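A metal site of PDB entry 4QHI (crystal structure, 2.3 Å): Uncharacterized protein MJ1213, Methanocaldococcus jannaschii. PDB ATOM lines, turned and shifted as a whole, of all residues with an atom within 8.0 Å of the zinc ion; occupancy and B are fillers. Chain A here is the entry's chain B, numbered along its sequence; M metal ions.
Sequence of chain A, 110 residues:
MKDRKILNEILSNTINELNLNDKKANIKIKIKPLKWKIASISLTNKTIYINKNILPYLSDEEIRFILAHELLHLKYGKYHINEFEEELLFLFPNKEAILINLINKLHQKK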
ATOM      1  N   HIS A  69     -13.779  -2.163 -19.793  1.00  0.00           N
ATOM      2  CA  HIS A  69     -12.936  -2.990 -18.949  1.00  0.00           C
ATOM      3  C   HIS A  69     -13.339  -2.833 -17.477  1.00  0.00           C
ATOM      4  O   HIS A  69     -13.563  -3.848 -16.820  1.00  0.00           O
ATOM      5  CB  HIS A  69     -11.447  -2.643 -19.148  1.00  0.00           C
ATOM      6  CG  HIS A  69     -10.540  -3.275 -18.126  1.00  0.00           C
ATOM      7  ND1 HIS A  69      -9.833  -2.514 -17.216  1.00  0.00           N
ATOM      8  CD2 HIS A  69     -10.353  -4.583 -17.832  1.00  0.00           C
ATOM      9  CE1 HIS A  69      -9.175  -3.375 -16.454  1.00  0.00           C
ATOM     10  NE2 HIS A  69      -9.461  -4.632 -16.793  1.00  0.00           N
ATOM     11  N   GLU A  70     -13.466  -1.588 -16.983  1.00  0.00           N
ATOM     12  CA  GLU A  70     -13.858  -1.246 -15.608  1.00  0.00           C
ATOM     13  C   GLU A  70     -15.266  -1.759 -15.298  1.00  0.00           C
ATOM     14  O   GLU A  70     -15.447  -2.391 -14.257  1.00  0.00           O
ATOM     15  CB  GLU A  70     -13.827   0.276 -15.391  1.00  0.00           C
ATOM     16  CG  GLU A  70     -12.434   0.892 -15.283  1.00  0.00           C
ATOM     17  CD  GLU A  70     -11.707   0.737 -13.963  1.00  0.00           C
ATOM     18  OE1 GLU A  70     -12.316   0.302 -12.965  1.00  0.00           O
ATOM     19  OE2 GLU A  70     -10.474   0.932 -13.979  1.00  0.00           O
ATOM     20  N   LEU A  72     -16.921  -4.142 -16.698  1.00  0.00           N
ATOM     21  CA  LEU A  72     -16.998  -5.594 -16.712  1.00  0.00           C
ATOM     22  C   LEU A  72     -16.548  -6.196 -15.372  1.00  0.00           C
ATOM     23  O   LEU A  72     -17.012  -7.287 -15.039  1.00  0.00           O
ATOM     24  CB  LEU A  72     -16.225  -6.164 -17.890  1.00  0.00           C
ATOM     25  CG  LEU A  72     -16.959  -6.150 -19.269  1.00  0.00           C
ATOM     26  CD1 LEU A  72     -16.027  -6.531 -20.388  1.00  0.00           C
ATOM     27  CD2 LEU A  72     -18.168  -7.063 -19.274  1.00  0.00           C
ATOM     28  N   HIS A  73     -15.727  -5.462 -14.565  1.00  0.00           N
ATOM     29  CA  HIS A  73     -15.317  -5.914 -13.231  1.00  0.00           C
ATOM     30  C   HIS A  73     -16.470  -5.783 -12.248  1.00  0.00           C
ATOM     31  O   HIS A  73     -16.537  -6.581 -11.316  1.00  0.00           O
ATOM     32  CB  HIS A  73     -14.072  -5.179 -12.732  1.00  0.00           C
ATOM     33  CG  HIS A  73     -12.796  -5.741 -13.292  1.00  0.00           C
ATOM     34  ND1 HIS A  73     -12.315  -6.987 -12.898  1.00  0.00           N
ATOM     35  CD2 HIS A  73     -11.951  -5.220 -14.206  1.00  0.00           C
ATOM     36  CE1 HIS A  73     -11.205  -7.191 -13.589  1.00  0.00           C
ATOM     37  NE2 HIS A  73     -10.936  -6.153 -14.380  1.00  0.00           N
ATOM     38  N   GLY A  77     -16.722  -9.507 -11.311  1.00  0.00           N
ATOM     39  CA  GLY A  77     -15.813  -9.595 -10.161  1.00  0.00           C
ATOM     40  C   GLY A  77     -14.419  -9.135 -10.525  1.00  0.00           C
ATOM     41  O   GLY A  77     -14.202  -8.620 -11.624  1.00  0.00           O
ATOM     42  N   LYS A  78     -13.472  -9.370  -9.599  1.00  0.00           N
ATOM     43  CA  LYS A  78     -12.106  -8.875  -9.754  1.00  0.00           C
ATOM     44  C   LYS A  78     -11.244  -9.658 -10.786  1.00  0.00           C
ATOM     45  O   LYS A  78     -10.170  -9.163 -11.147  1.00  0.00           O
ATOM     46  CB  LYS A  78     -11.386  -8.796  -8.393  1.00  0.00           C
ATOM     47  CG  LYS A  78     -11.102 -10.112  -7.677  1.00  0.00           C
ATOM     48  CD  LYS A  78     -10.145  -9.922  -6.472  1.00  0.00           C
ATOM     49  CE  LYS A  78      -8.725  -9.541  -6.847  1.00  0.00           C
ATOM     50  NZ  LYS A  78      -7.800  -9.664  -5.681  1.00  0.00           N
ATOM     51  N   TYR A  79     -11.702 -10.810 -11.301  1.00  0.00           N
ATOM     52  CA  TYR A  79     -10.892 -11.605 -12.243  1.00  0.00           C
ATOM     53  C   TYR A  79     -11.427 -11.643 -13.679  1.00  0.00           C
ATOM     54  O   TYR A  79     -12.633 -11.616 -13.912  1.00  0.00           O
ATOM     55  CB  TYR A  79     -10.692 -13.023 -11.704  1.00  0.00           C
ATOM     56  CG  TYR A  79      -9.991 -13.018 -10.376  1.00  0.00           C
ATOM     57  CD1 TYR A  79      -8.677 -12.557 -10.253  1.00  0.00           C
ATOM     58  CD2 TYR A  79     -10.652 -13.394  -9.218  1.00  0.00           C
ATOM     59  CE1 TYR A  79      -8.041 -12.501  -9.019  1.00  0.00           C
ATOM     60  CE2 TYR A  79     -10.022 -13.374  -7.973  1.00  0.00           C
ATOM     61  CZ  TYR A  79      -8.707 -12.919  -7.882  1.00  0.00           C
ATOM     62  OH  TYR A  79      -8.077 -12.891  -6.658  1.00  0.00           O
ATOM     63  N   HIS A  80     -10.494 -11.715 -14.631  1.00  0.00           N
ATOM     64  CA  HIS A  80     -10.774 -11.785 -16.057  1.00  0.00           C
ATOM     65  C   HIS A  80     -11.180 -13.207 -16.435  1.00  0.00           C
ATOM     66  O   HIS A  80     -10.453 -13.893 -17.165  1.00  0.00           O
ATOM     67  CB  HIS A  80      -9.556 -11.296 -16.866  1.00  0.00           C
ATOM     68  CG  HIS A  80      -9.085  -9.929 -16.479  1.00  0.00           C
ATOM     69  ND1 HIS A  80      -7.769  -9.696 -16.162  1.00  0.00           N
ATOM     70  CD2 HIS A  80      -9.763  -8.760 -16.396  1.00  0.00           C
ATOM     71  CE1 HIS A  80      -7.683  -8.411 -15.890  1.00  0.00           C
ATOM     72  NE2 HIS A  80      -8.860  -7.803 -16.000  1.00  0.00           N
ATOM     73  N   PHE A  84     -15.887 -12.567 -19.077  1.00  0.00           N
ATOM     74  CA  PHE A  84     -15.332 -11.213 -19.124  1.00  0.00           C
ATOM     75  C   PHE A  84     -14.638 -10.984 -20.486  1.00  0.00           C
ATOM     76  O   PHE A  84     -14.955 -10.032 -21.208  1.00  0.00           O
ATOM     77  CB  PHE A  84     -14.328 -11.004 -17.958  1.00  0.00           C
ATOM     78  CG  PHE A  84     -13.790  -9.605 -17.719  1.00  0.00           C
ATOM     79  CD1 PHE A  84     -13.016  -8.960 -18.688  1.00  0.00           C
ATOM     80  CD2 PHE A  84     -14.005  -8.945 -16.513  1.00  0.00           C
ATOM     81  CE1 PHE A  84     -12.524  -7.650 -18.481  1.00  0.00           C
ATOM     82  CE2 PHE A  84     -13.493  -7.656 -16.289  1.00  0.00           C
ATOM     83  CZ  PHE A  84     -12.768  -7.019 -17.282  1.00  0.00           C
ATOM     84  N   LEU A  88     -15.831  -8.563 -23.714  1.00  0.00           N
ATOM     85  CA  LEU A  88     -14.897  -7.536 -24.153  1.00  0.00           C
ATOM     86  C   LEU A  88     -14.484  -7.769 -25.629  1.00  0.00           C
ATOM     87  O   LEU A  88     -14.379  -6.813 -26.380  1.00  0.00           O
ATOM     88  CB  LEU A  88     -13.660  -7.475 -23.228  1.00  0.00           C
ATOM     89  CG  LEU A  88     -12.831  -6.182 -23.227  1.00  0.00           C
ATOM     90  CD1 LEU A  88     -13.711  -4.951 -22.963  1.00  0.00           C
ATOM     91  CD2 LEU A  88     -11.755  -6.236 -22.198  1.00  0.00           C
ATOM     92  N   ILE A 100      -5.815  -9.058 -23.875  1.00  0.00           N
ATOM     93  CA  ILE A 100      -5.322  -9.517 -22.569  1.00  0.00           C
ATOM     94  C   ILE A 100      -4.183  -8.620 -22.074  1.00  0.00           C
ATOM     95  O   ILE A 100      -4.233  -8.223 -20.907  1.00  0.00           O
ATOM     96  CB  ILE A 100      -4.940 -11.027 -22.568  1.00  0.00           C
ATOM     97  CG1 ILE A 100      -6.106 -11.892 -23.124  1.00  0.00           C
ATOM     98  CG2 ILE A 100      -4.511 -11.516 -21.175  1.00  0.00           C
ATOM     99  CD1 ILE A 100      -7.453 -11.816 -22.370  1.00  0.00           C
ATOM    100  N   LEU A 102      -3.617  -5.498 -22.758  1.00  0.00           N
ATOM    101  CA  LEU A 102      -4.183  -4.208 -22.419  1.00  0.00           C
ATOM    102  C   LEU A 102      -4.896  -4.233 -21.080  1.00  0.00           C
ATOM    103  O   LEU A 102      -4.590  -3.383 -20.254  1.00  0.00           O
ATOM    104  CB  LEU A 102      -5.133  -3.694 -23.511  1.00  0.00           C
ATOM    105  CG  LEU A 102      -4.472  -3.354 -24.865  1.00  0.00           C
ATOM    106  CD1 LEU A 102      -5.491  -2.819 -25.832  1.00  0.00           C
ATOM    107  CD2 LEU A 102      -3.341  -2.361 -24.697  1.00  0.00           C
ATOM    108  N   ILE A 103      -5.753  -5.244 -20.838  1.00  0.00           N
ATOM    109  CA  ILE A 103      -6.530  -5.335 -19.608  1.00  0.00           C
ATOM    110  C   ILE A 103      -5.615  -5.631 -18.419  1.00  0.00           C
ATOM    111  O   ILE A 103      -5.806  -5.022 -17.371  1.00  0.00           O
ATOM    112  CB  ILE A 103      -7.764  -6.266 -19.703  1.00  0.00           C
ATOM    113  CG1 ILE A 103      -7.400  -7.747 -19.926  1.00  0.00           C
ATOM    114  CG2 ILE A 103      -8.697  -5.728 -20.781  1.00  0.00           C
ATOM    115  CD1 ILE A 103      -8.585  -8.734 -19.901  1.00  0.00           C
ATOM    116  N   ASN A 104      -4.570  -6.447 -18.609  1.00  0.00           N
ATOM    117  CA  ASN A 104      -3.590  -6.748 -17.567  1.00  0.00           C
ATOM    118  C   ASN A 104      -2.787  -5.500 -17.177  1.00  0.00           C
ATOM    119  O   ASN A 104      -2.506  -5.310 -15.984  1.00  0.00           O
ATOM    120  CB  ASN A 104      -2.637  -7.866 -18.002  1.00  0.00           C
ATOM    121  CG  ASN A 104      -3.196  -9.275 -17.861  1.00  0.00           C
ATOM    122  OD1 ASN A 104      -4.220  -9.517 -17.214  1.00  0.00           O
ATOM    123  ND2 ASN A 104      -2.506 -10.235 -18.468  1.00  0.00           N
ATOM    124  N   LYS A 105      -2.448  -4.642 -18.150  1.00  0.00           N
ATOM    125  CA  LYS A 105      -1.673  -3.417 -17.923  1.00  0.00           C
ATOM    126  C   LYS A 105      -2.544  -2.268 -17.322  1.00  0.00           C
ATOM    127  O   LYS A 105      -2.022  -1.199 -17.004  1.00  0.00           O
ATOM    128  CB  LYS A 105      -0.978  -2.956 -19.220  1.00  0.00           C
ATOM    129  CG  LYS A 105       0.111  -3.874 -19.716  1.00  0.00           C
ATOM    130  CD  LYS A 105       1.499  -3.455 -19.229  1.00  0.00           C
ATOM    131  CE  LYS A 105       2.580  -4.370 -19.749  1.00  0.00           C
ATOM    132  NZ  LYS A 105       2.737  -4.270 -21.225  1.00  0.00           N
ATOM    133  N   LEU A 106      -3.837  -2.499 -17.134  1.00  0.00           N
ATOM    134  CA  LEU A 106      -4.740  -1.494 -16.589  1.00  0.00           C
ATOM    135  C   LEU A 106      -4.923  -1.662 -15.087  1.00  0.00           C
ATOM    136  O   LEU A 106      -5.670  -0.892 -14.469  1.00  0.00           O
ATOM    137  CB  LEU A 106      -6.102  -1.529 -17.321  1.00  0.00           C
ATOM    138  CG  LEU A 106      -6.093  -0.836 -18.712  1.00  0.00           C
ATOM    139  CD1 LEU A 106      -7.244  -1.324 -19.588  1.00  0.00           C
ATOM    140  CD2 LEU A 106      -6.117   0.667 -18.561  1.00  0.00           C
ATOM    141  N   HIS A 107      -4.233  -2.642 -14.498  1.00  0.00           N
ATOM    142  CA  HIS A 107      -4.299  -2.933 -13.073  1.00  0.00           C
ATOM    143  C   HIS A 107      -3.079  -2.382 -12.377  1.00  0.00           C
ATOM    144  O   HIS A 107      -1.948  -2.580 -12.845  1.00  0.00           O
ATOM    145  CB  HIS A 107      -4.474  -4.435 -12.822  1.00  0.00           C
ATOM    146  CG  HIS A 107      -5.824  -4.912 -13.235  1.00  0.00           C
ATOM    147  ND1 HIS A 107      -6.897  -4.863 -12.372  1.00  0.00           N
ATOM    148  CD2 HIS A 107      -6.255  -5.324 -14.442  1.00  0.00           C
ATOM    149  CE1 HIS A 107      -7.945  -5.285 -13.066  1.00  0.00           C
ATOM    150  NE2 HIS A 107      -7.608  -5.565 -14.323  1.00  0.00           N
HETATM  151 ZN    ZN M   1      -9.186  -6.011 -15.392  1.00  0.00          ZN
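ND1 of His 73 lies within hydrogen-bond range of O of Gly 77 (2.8 Å).
Within 4 Å of the zinc ion: His 69, His 73, His 80 and His 107.
The zinc ion is bound by a ring nitrogen (NE2) of His 80 (1.9 Å), a ring nitrogen (NE2) of His 107 (2.0 Å), a ring nitrogen (NE2) of His 69 (2.0 Å) and a ring nitrogen (NE2) of His 73 (2.0 Å).
The zinc ion has four donor atoms within binding distance.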
